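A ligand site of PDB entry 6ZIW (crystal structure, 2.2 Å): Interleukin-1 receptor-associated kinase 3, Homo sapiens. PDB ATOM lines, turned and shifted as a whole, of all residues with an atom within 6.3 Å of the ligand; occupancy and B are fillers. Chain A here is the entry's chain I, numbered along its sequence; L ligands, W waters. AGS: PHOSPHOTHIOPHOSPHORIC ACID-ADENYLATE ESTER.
Water W1 bridges OD1 of Asp 172 (2.7 Å) and O2G of the ligand (3.1 Å).
Merely in contact with the ligand: Ile 32, Gly 33, Glu 34, Gly 35, Val 40, Ala 51, Leu 86, Tyr 102, Tyr 104, Thr 109 and Leu 161.
Of the 28 residues printed, 18 come within 4 Å of the ligand.
The nearest printed residue that does not touch the ligand is Asn 159 (4.8 Å).
The side-chain carboxylate (OD2) of Asp 172 sits at hydrogen-bond distance from the backbone NH (N) of Ala 174 (3.1 Å).
O of Ile 37 lies within hydrogen-bond range of N of Lys 56, 3.1 Å away.
The backbone carbonyl oxygen of Val 40 sits at hydrogen-bond distance from the backbone NH of Ile 32, at 2.7 Å.
The backbone carbonyl oxygen (O) of Gly 33 sits at hydrogen-bond distance from the backbone NH (N) of Val 40, 3.0 Å away.
N of Asp 112 is in hydrogen-bond range of OG1 of Thr 109 (2.9 Å).
N of Ala 51 sits at hydrogen-bond distance from O of Tyr 102.
NZ of Lys 56 sits at hydrogen-bond distance from O of Gly 35.
OE1 of Glu 34 lies within salt-bridge range of NZ of Lys 56.
The side-chain amino group (NZ) of Lys 53 lies within salt-bridge range of an oxygen (O2B) of the ligand, 2.4 Å away.
The backbone NH (N) of Phe 38 is in hydrogen-bond range of an oxygen (O1B) of the ligand, 2.9 Å away.
A nitrogen (N6) of the ligand lies within hydrogen-bond range of the backbone carbonyl oxygen (O) of Pro 103, 3.0 Å away.
The backbone NH (N) of Met 105 sits at hydrogen-bond distance from a nitrogen (N1) of the ligand (3.1 Å).
O2G of the ligand lies within hydrogen-bond range of OD1 of Asp 172 (3.3 Å).
O1B of the ligand sits at hydrogen-bond distance from N of Ile 37.
An oxygen (O3G) of the ligand sits at hydrogen-bond distance from the backbone NH of Glu 36 (3.3 Å).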
ATOM      1  N   ILE A  32      21.703 -19.940  19.110  1.00  0.00           N
ATOM      2  CA  ILE A  32      22.283 -20.658  17.966  1.00  0.00           C
ATOM      3  C   ILE A  32      21.287 -21.635  17.375  1.00  0.00           C
ATOM      4  O   ILE A  32      21.072 -21.678  16.164  1.00  0.00           O
ATOM      5  CB  ILE A  32      23.575 -21.381  18.405  1.00  0.00           C
ATOM      6  CG1 ILE A  32      24.633 -20.373  18.829  1.00  0.00           C
ATOM      7  CG2 ILE A  32      24.129 -22.230  17.287  1.00  0.00           C
ATOM      8  CD1 ILE A  32      25.874 -21.061  19.303  1.00  0.00           C
ATOM      9  N   GLY A  33      20.672 -22.452  18.232  1.00  0.00           N
ATOM     10  CA  GLY A  33      19.742 -23.470  17.775  1.00  0.00           C
ATOM     11  C   GLY A  33      19.312 -24.311  18.943  1.00  0.00           C
ATOM     12  O   GLY A  33      19.526 -23.941  20.102  1.00  0.00           O
ATOM     13  N   GLU A  34      18.714 -25.462  18.637  1.00  0.00           N
ATOM     14  CA  GLU A  34      18.211 -26.366  19.675  1.00  0.00           C
ATOM     15  C   GLU A  34      18.006 -27.761  19.101  1.00  0.00           C
ATOM     16  O   GLU A  34      17.459 -27.914  18.002  1.00  0.00           O
ATOM     17  CB  GLU A  34      16.895 -25.851  20.270  1.00  0.00           C
ATOM     18  CG  GLU A  34      16.385 -26.713  21.399  1.00  0.00           C
ATOM     19  CD  GLU A  34      15.087 -26.200  21.982  1.00  0.00           C
ATOM     20  OE1 GLU A  34      14.245 -27.035  22.407  1.00  0.00           O
ATOM     21  OE2 GLU A  34      14.902 -24.968  22.010  1.00  0.00           O
ATOM     22  N   GLY A  35      18.460 -28.772  19.845  1.00  0.00           N
ATOM     23  CA  GLY A  35      18.216 -30.161  19.496  1.00  0.00           C
ATOM     24  C   GLY A  35      17.281 -30.859  20.477  1.00  0.00           C
ATOM     25  O   GLY A  35      16.399 -30.215  21.072  1.00  0.00           O
ATOM     26  N   GLU A  36      17.476 -32.171  20.672  1.00  0.00           N
ATOM     27  CA  GLU A  36      16.616 -32.953  21.544  1.00  0.00           C
ATOM     28  C   GLU A  36      16.947 -32.804  23.029  1.00  0.00           C
ATOM     29  O   GLU A  36      16.034 -32.856  23.866  1.00  0.00           O
ATOM     30  CB  GLU A  36      16.686 -34.435  21.155  1.00  0.00           C
ATOM     31  N   ILE A  37      18.222 -32.601  23.378  1.00  0.00           N
ATOM     32  CA  ILE A  37      18.625 -32.512  24.773  1.00  0.00           C
ATOM     33  C   ILE A  37      19.045 -31.104  25.210  1.00  0.00           C
ATOM     34  O   ILE A  37      19.076 -30.846  26.431  1.00  0.00           O
ATOM     35  CB  ILE A  37      19.746 -33.524  25.091  1.00  0.00           C
ATOM     36  N   PHE A  38      19.358 -30.189  24.283  1.00  0.00           N
ATOM     37  CA  PHE A  38      19.959 -28.902  24.641  1.00  0.00           C
ATOM     38  C   PHE A  38      19.364 -27.722  23.869  1.00  0.00           C
ATOM     39  O   PHE A  38      19.086 -27.837  22.664  1.00  0.00           O
ATOM     40  CB  PHE A  38      21.478 -28.912  24.422  1.00  0.00           C
ATOM     41  CG  PHE A  38      22.205 -30.008  25.162  1.00  0.00           C
ATOM     42  CD1 PHE A  38      22.518 -31.211  24.534  1.00  0.00           C
ATOM     43  CD2 PHE A  38      22.569 -29.832  26.502  1.00  0.00           C
ATOM     44  CE1 PHE A  38      23.193 -32.218  25.215  1.00  0.00           C
ATOM     45  CE2 PHE A  38      23.238 -30.839  27.199  1.00  0.00           C
ATOM     46  CZ  PHE A  38      23.559 -32.033  26.550  1.00  0.00           C
ATOM     47  N   GLU A  39      19.201 -26.589  24.559  1.00  0.00           N
ATOM     48  CA  GLU A  39      19.101 -25.274  23.934  1.00  0.00           C
ATOM     49  C   GLU A  39      20.489 -24.643  23.903  1.00  0.00           C
ATOM     50  O   GLU A  39      21.208 -24.684  24.916  1.00  0.00           O
ATOM     51  CB  GLU A  39      18.113 -24.379  24.687  1.00  0.00           C
ATOM     52  N   VAL A  40      20.855 -24.050  22.765  1.00  0.00           N
ATOM     53  CA  VAL A  40      22.252 -23.700  22.489  1.00  0.00           C
ATOM     54  C   VAL A  40      22.371 -22.210  22.169  1.00  0.00           C
ATOM     55  O   VAL A  40      21.778 -21.719  21.201  1.00  0.00           O
ATOM     56  CB  VAL A  40      22.827 -24.528  21.337  1.00  0.00           C
ATOM     57  CG1 VAL A  40      24.286 -24.171  21.129  1.00  0.00           C
ATOM     58  CG2 VAL A  40      22.649 -26.016  21.608  1.00  0.00           C
ATOM     59  N   TYR A  50      31.991 -18.823  23.042  1.00  0.00           N
ATOM     60  CA  TYR A  50      31.576 -20.156  23.443  1.00  0.00           C
ATOM     61  C   TYR A  50      30.170 -20.449  22.925  1.00  0.00           C
ATOM     62  O   TYR A  50      29.421 -19.554  22.535  1.00  0.00           O
ATOM     63  CB  TYR A  50      31.572 -20.322  24.989  1.00  0.00           C
ATOM     64  CG  TYR A  50      32.944 -20.176  25.608  1.00  0.00           C
ATOM     65  CD1 TYR A  50      33.374 -18.953  26.078  1.00  0.00           C
ATOM     66  CD2 TYR A  50      33.828 -21.245  25.653  1.00  0.00           C
ATOM     67  CE1 TYR A  50      34.638 -18.797  26.615  1.00  0.00           C
ATOM     68  CE2 TYR A  50      35.089 -21.112  26.187  1.00  0.00           C
ATOM     69  CZ  TYR A  50      35.493 -19.885  26.674  1.00  0.00           C
ATOM     70  OH  TYR A  50      36.746 -19.716  27.226  1.00  0.00           O
ATOM     71  N   ALA A  51      29.843 -21.741  22.938  1.00  0.00           N
ATOM     72  CA  ALA A  51      28.473 -22.239  22.770  1.00  0.00           C
ATOM     73  C   ALA A  51      28.083 -22.940  24.063  1.00  0.00           C
ATOM     74  O   ALA A  51      28.808 -23.832  24.531  1.00  0.00           O
ATOM     75  CB  ALA A  51      28.381 -23.199  21.575  1.00  0.00           C
ATOM     76  N   LYS A  53      25.264 -25.253  25.910  1.00  0.00           N
ATOM     77  CA  LYS A  53      24.204 -26.199  25.617  1.00  0.00           C
ATOM     78  C   LYS A  53      23.411 -26.361  26.915  1.00  0.00           C
ATOM     79  O   LYS A  53      23.886 -26.972  27.880  1.00  0.00           O
ATOM     80  CB  LYS A  53      24.818 -27.499  25.083  1.00  0.00           C
ATOM     81  CG  LYS A  53      25.380 -27.353  23.632  1.00  0.00           C
ATOM     82  CD  LYS A  53      26.365 -28.467  23.185  1.00  0.00           C
ATOM     83  CE  LYS A  53      25.789 -29.872  22.966  1.00  0.00           C
ATOM     84  NZ  LYS A  53      24.905 -30.113  21.762  1.00  0.00           N
ATOM     85  N   LYS A  56      17.921 -29.406  28.878  1.00  0.00           N
ATOM     86  CA  LYS A  56      16.518 -29.026  28.824  1.00  0.00           C
ATOM     87  C   LYS A  56      15.611 -29.921  29.681  1.00  0.00           C
ATOM     88  O   LYS A  56      14.987 -29.458  30.642  1.00  0.00           O
ATOM     89  CB  LYS A  56      16.101 -29.057  27.356  1.00  0.00           C
ATOM     90  CG  LYS A  56      15.123 -28.010  26.903  1.00  0.00           C
ATOM     91  CD  LYS A  56      15.241 -27.917  25.394  1.00  0.00           C
ATOM     92  CE  LYS A  56      15.308 -29.321  24.802  1.00  0.00           C
ATOM     93  NZ  LYS A  56      15.401 -29.345  23.325  1.00  0.00           N
ATOM     94  N   LEU A  86      36.100 -31.832  20.020  1.00  0.00           N
ATOM     95  CA  LEU A  86      35.751 -30.560  20.648  1.00  0.00           C
ATOM     96  C   LEU A  86      35.695 -30.725  22.167  1.00  0.00           C
ATOM     97  O   LEU A  86      34.953 -31.565  22.703  1.00  0.00           O
ATOM     98  CB  LEU A  86      34.415 -30.054  20.114  1.00  0.00           C
ATOM     99  CG  LEU A  86      34.127 -28.626  20.608  1.00  0.00           C
ATOM    100  CD1 LEU A  86      35.227 -27.678  20.119  1.00  0.00           C
ATOM    101  CD2 LEU A  86      32.768 -28.130  20.193  1.00  0.00           C
ATOM    102  N   TYR A 102      31.291 -25.270  25.476  1.00  0.00           N
ATOM    103  CA  TYR A 102      32.319 -25.654  24.514  1.00  0.00           C
ATOM    104  C   TYR A 102      32.847 -24.428  23.771  1.00  0.00           C
ATOM    105  O   TYR A 102      32.123 -23.437  23.608  1.00  0.00           O
ATOM    106  CB  TYR A 102      31.801 -26.646  23.454  1.00  0.00           C
ATOM    107  CG  TYR A 102      31.012 -27.840  23.946  1.00  0.00           C
ATOM    108  CD1 TYR A 102      29.699 -27.703  24.396  1.00  0.00           C
ATOM    109  CD2 TYR A 102      31.542 -29.119  23.891  1.00  0.00           C
ATOM    110  CE1 TYR A 102      28.975 -28.819  24.829  1.00  0.00           C
ATOM    111  CE2 TYR A 102      30.813 -30.238  24.315  1.00  0.00           C
ATOM    112  CZ  TYR A 102      29.531 -30.072  24.771  1.00  0.00           C
ATOM    113  OH  TYR A 102      28.810 -31.181  25.175  1.00  0.00           O
ATOM    114  N   PRO A 103      34.087 -24.467  23.287  1.00  0.00           N
ATOM    115  CA  PRO A 103      34.575 -23.381  22.420  1.00  0.00           C
ATOM    116  C   PRO A 103      33.690 -23.263  21.177  1.00  0.00           C
ATOM    117  O   PRO A 103      33.240 -24.269  20.618  1.00  0.00           O
ATOM    118  CB  PRO A 103      36.002 -23.809  22.059  1.00  0.00           C
ATOM    119  CG  PRO A 103      36.372 -24.871  23.029  1.00  0.00           C
ATOM    120  CD  PRO A 103      35.098 -25.508  23.513  1.00  0.00           C
ATOM    121  N   TYR A 104      33.458 -22.021  20.755  1.00  0.00           N
ATOM    122  CA  TYR A 104      32.591 -21.758  19.612  1.00  0.00           C
ATOM    123  C   TYR A 104      33.327 -22.044  18.310  1.00  0.00           C
ATOM    124  O   TYR A 104      34.461 -21.601  18.102  1.00  0.00           O
ATOM    125  CB  TYR A 104      32.080 -20.318  19.648  1.00  0.00           C
ATOM    126  CG  TYR A 104      31.074 -20.002  18.569  1.00  0.00           C
ATOM    127  CD1 TYR A 104      29.715 -20.304  18.739  1.00  0.00           C
ATOM    128  CD2 TYR A 104      31.458 -19.382  17.384  1.00  0.00           C
ATOM    129  CE1 TYR A 104      28.787 -20.018  17.755  1.00  0.00           C
ATOM    130  CE2 TYR A 104      30.527 -19.092  16.363  1.00  0.00           C
ATOM    131  CZ  TYR A 104      29.185 -19.416  16.567  1.00  0.00           C
ATOM    132  OH  TYR A 104      28.252 -19.131  15.600  1.00  0.00           O
ATOM    133  N   MET A 105      32.671 -22.783  17.417  1.00  0.00           N
ATOM    134  CA  MET A 105      33.284 -23.247  16.173  1.00  0.00           C
ATOM    135  C   MET A 105      32.696 -22.396  15.048  1.00  0.00           C
ATOM    136  O   MET A 105      31.564 -22.620  14.610  1.00  0.00           O
ATOM    137  CB  MET A 105      32.995 -24.735  16.003  1.00  0.00           C
ATOM    138  CG  MET A 105      33.895 -25.716  16.787  1.00  0.00           C
ATOM    139  SD  MET A 105      35.691 -25.506  16.731  1.00  0.00           S
ATOM    140  CE  MET A 105      36.072 -24.331  18.044  1.00  0.00           C
ATOM    141  N   ARG A 106      33.461 -21.410  14.596  1.00  0.00           N
ATOM    142  CA  ARG A 106      32.948 -20.356  13.726  1.00  0.00           C
ATOM    143  C   ARG A 106      32.643 -20.844  12.306  1.00  0.00           C
ATOM    144  O   ARG A 106      31.807 -20.245  11.614  1.00  0.00           O
ATOM    145  CB  ARG A 106      33.961 -19.205  13.702  1.00  0.00           C
ATOM    146  CG  ARG A 106      33.378 -17.821  13.706  1.00  0.00           C
ATOM    147  CD  ARG A 106      34.456 -16.766  14.012  1.00  0.00           C
ATOM    148  NE  ARG A 106      34.644 -16.535  15.439  1.00  0.00           N
ATOM    149  CZ  ARG A 106      33.765 -15.870  16.200  1.00  0.00           C
ATOM    150  NH1 ARG A 106      32.654 -15.378  15.657  1.00  0.00           N
ATOM    151  NH2 ARG A 106      34.003 -15.681  17.494  1.00  0.00           N
ATOM    152  N   GLY A 108      31.187 -23.661  11.736  1.00  0.00           N
ATOM    153  CA  GLY A 108      29.967 -24.469  11.753  1.00  0.00           C
ATOM    154  C   GLY A 108      30.210 -25.961  11.502  1.00  0.00           C
ATOM    155  O   GLY A 108      31.290 -26.509  11.759  1.00  0.00           O
ATOM    156  N   THR A 109      29.153 -26.618  11.028  1.00  0.00           N
ATOM    157  CA  THR A 109      29.138 -28.060  10.833  1.00  0.00           C
ATOM    158  C   THR A 109      29.567 -28.429   9.428  1.00  0.00           C
ATOM    159  O   THR A 109      29.356 -27.668   8.470  1.00  0.00           O
ATOM    160  CB  THR A 109      27.744 -28.642  11.077  1.00  0.00           C
ATOM    161  OG1 THR A 109      26.892 -28.294   9.969  1.00  0.00           O
ATOM    162  CG2 THR A 109      27.144 -28.129  12.395  1.00  0.00           C
ATOM    163  N   ASP A 112      26.603 -28.191   7.070  1.00  0.00           N
ATOM    164  CA  ASP A 112      26.295 -26.846   6.600  1.00  0.00           C
ATOM    165  C   ASP A 112      27.249 -26.409   5.497  1.00  0.00           C
ATOM    166  O   ASP A 112      26.830 -25.736   4.548  1.00  0.00           O
ATOM    167  CB  ASP A 112      26.362 -25.860   7.765  1.00  0.00           C
ATOM    168  CG  ASP A 112      25.088 -25.815   8.560  1.00  0.00           C
ATOM    169  OD1 ASP A 112      24.203 -26.654   8.299  1.00  0.00           O
ATOM    170  OD2 ASP A 112      24.954 -24.940   9.461  1.00  0.00           O
ATOM    171  N   ALA A 158      26.644 -33.569  10.524  1.00  0.00           N
ATOM    172  CA  ALA A 158      26.135 -32.575  11.459  1.00  0.00           C
ATOM    173  C   ALA A 158      26.983 -32.483  12.715  1.00  0.00           C
ATOM    174  O   ALA A 158      27.114 -31.403  13.300  1.00  0.00           O
ATOM    175  CB  ALA A 158      24.683 -32.901  11.853  1.00  0.00           C
ATOM    176  N   ASN A 159      27.556 -33.594  13.175  1.00  0.00           N
ATOM    177  CA  ASN A 159      28.266 -33.622  14.441  1.00  0.00           C
ATOM    178  C   ASN A 159      29.764 -33.368  14.281  1.00  0.00           C
ATOM    179  O   ASN A 159      30.520 -33.529  15.249  1.00  0.00           O
ATOM    180  CB  ASN A 159      28.017 -34.948  15.155  1.00  0.00           C
ATOM    181  CG  ASN A 159      26.587 -35.065  15.661  1.00  0.00           C
ATOM    182  OD1 ASN A 159      25.978 -34.072  16.073  1.00  0.00           O
ATOM    183  ND2 ASN A 159      26.045 -36.280  15.653  1.00  0.00           N
ATOM    184  N   LEU A 161      32.227 -30.380  13.706  1.00  0.00           N
ATOM    185  CA  LEU A 161      32.330 -28.929  13.688  1.00  0.00           C
ATOM    186  C   LEU A 161      33.703 -28.514  13.178  1.00  0.00           C
ATOM    187  O   LEU A 161      34.640 -29.314  13.118  1.00  0.00           O
ATOM    188  CB  LEU A 161      32.078 -28.340  15.097  1.00  0.00           C
ATOM    189  CG  LEU A 161      30.737 -28.652  15.788  1.00  0.00           C
ATOM    190  CD1 LEU A 161      30.533 -27.885  17.138  1.00  0.00           C
ATOM    191  CD2 LEU A 161      29.609 -28.349  14.832  1.00  0.00           C
ATOM    192  N   THR A 171      32.089 -34.148  17.742  1.00  0.00           N
ATOM    193  CA  THR A 171      31.204 -33.808  18.850  1.00  0.00           C
ATOM    194  C   THR A 171      30.126 -34.873  18.950  1.00  0.00           C
ATOM    195  O   THR A 171      29.969 -35.724  18.062  1.00  0.00           O
ATOM    196  CB  THR A 171      30.515 -32.442  18.679  1.00  0.00           C
ATOM    197  OG1 THR A 171      29.501 -32.518  17.656  1.00  0.00           O
ATOM    198  CG2 THR A 171      31.532 -31.344  18.307  1.00  0.00           C
ATOM    199  N   ASP A 172      29.364 -34.783  20.037  1.00  0.00           N
ATOM    200  CA  ASP A 172      28.208 -35.613  20.346  1.00  0.00           C
ATOM    201  C   ASP A 172      28.599 -37.011  20.767  1.00  0.00           C
ATOM    202  O   ASP A 172      28.710 -37.914  19.930  1.00  0.00           O
ATOM    203  CB  ASP A 172      27.238 -35.734  19.183  1.00  0.00           C
ATOM    204  CG  ASP A 172      25.876 -36.256  19.635  1.00  0.00           C
ATOM    205  OD1 ASP A 172      24.873 -35.975  18.943  1.00  0.00           O
ATOM    206  OD2 ASP A 172      25.804 -36.866  20.731  1.00  0.00           O
ATOM    207  N   ALA A 174      26.649 -38.461  23.230  1.00  0.00           N
ATOM    208  CA  ALA A 174      25.473 -38.860  24.003  1.00  0.00           C
ATOM    209  C   ALA A 174      25.114 -40.319  23.782  1.00  0.00           C
ATOM    210  O   ALA A 174      24.449 -40.912  24.632  1.00  0.00           O
ATOM    211  CB  ALA A 174      24.284 -37.971  23.662  1.00  0.00           C
HETATM  212  PG  AGS L   1      20.894 -33.744  19.610  1.00  0.00           P
HETATM  213  S1G AGS L   1      20.496 -34.416  21.351  1.00  0.00           S
HETATM  214  O2G AGS L   1      21.920 -34.561  18.740  1.00  0.00           O
HETATM  215  O3G AGS L   1      19.689 -33.576  18.604  1.00  0.00           O
HETATM  216  PB  AGS L   1      21.849 -31.297  20.902  1.00  0.00           P
HETATM  217  O1B AGS L   1      20.748 -31.096  21.878  1.00  0.00           O
HETATM  218  O2B AGS L   1      23.172 -31.795  21.505  1.00  0.00           O
HETATM  219  O3B AGS L   1      21.485 -32.279  19.710  1.00  0.00           O
HETATM  220  PA  AGS L   1      22.501 -29.609  18.591  1.00  0.00           P
HETATM  221  O1A AGS L   1      21.316 -29.734  17.688  1.00  0.00           O
HETATM  222  O2A AGS L   1      23.724 -30.462  18.230  1.00  0.00           O
HETATM  223  O3A AGS L   1      22.150 -29.939  20.103  1.00  0.00           O
HETATM  224  O5' AGS L   1      22.941 -28.100  18.689  1.00  0.00           O
HETATM  225  C5' AGS L   1      22.094 -27.001  18.293  1.00  0.00           C
HETATM  226  C4' AGS L   1      22.875 -26.111  17.360  1.00  0.00           C
HETATM  227  O4' AGS L   1      24.029 -25.559  18.058  1.00  0.00           O
HETATM  228  C3' AGS L   1      23.414 -26.815  16.113  1.00  0.00           C
HETATM  229  O3' AGS L   1      23.176 -25.993  14.976  1.00  0.00           O
HETATM  230  C2' AGS L   1      24.907 -27.000  16.415  1.00  0.00           C
HETATM  231  O2' AGS L   1      25.764 -26.992  15.279  1.00  0.00           O
HETATM  232  C1' AGS L   1      25.188 -25.762  17.258  1.00  0.00           C
HETATM  233  N9  AGS L   1      26.362 -25.883  18.118  1.00  0.00           N
HETATM  234  C8  AGS L   1      26.570 -26.747  19.164  1.00  0.00           C
HETATM  235  N7  AGS L   1      27.776 -26.678  19.683  1.00  0.00           N
HETATM  236  C5  AGS L   1      28.403 -25.702  18.925  1.00  0.00           C
HETATM  237  C6  AGS L   1      29.696 -25.136  18.982  1.00  0.00           C
HETATM  238  N6  AGS L   1      30.659 -25.563  19.816  1.00  0.00           N
HETATM  239  N1  AGS L   1      29.979 -24.128  18.118  1.00  0.00           N
HETATM  240  C2  AGS L   1      29.035 -23.733  17.257  1.00  0.00           C
HETATM  241  N3  AGS L   1      27.801 -24.197  17.099  1.00  0.00           N
HETATM  242  C4  AGS L   1      27.531 -25.190  17.974  1.00  0.00           C
HETATM  243  O   HOH W   1      22.769 -37.250  20.064  1.00  0.00           O
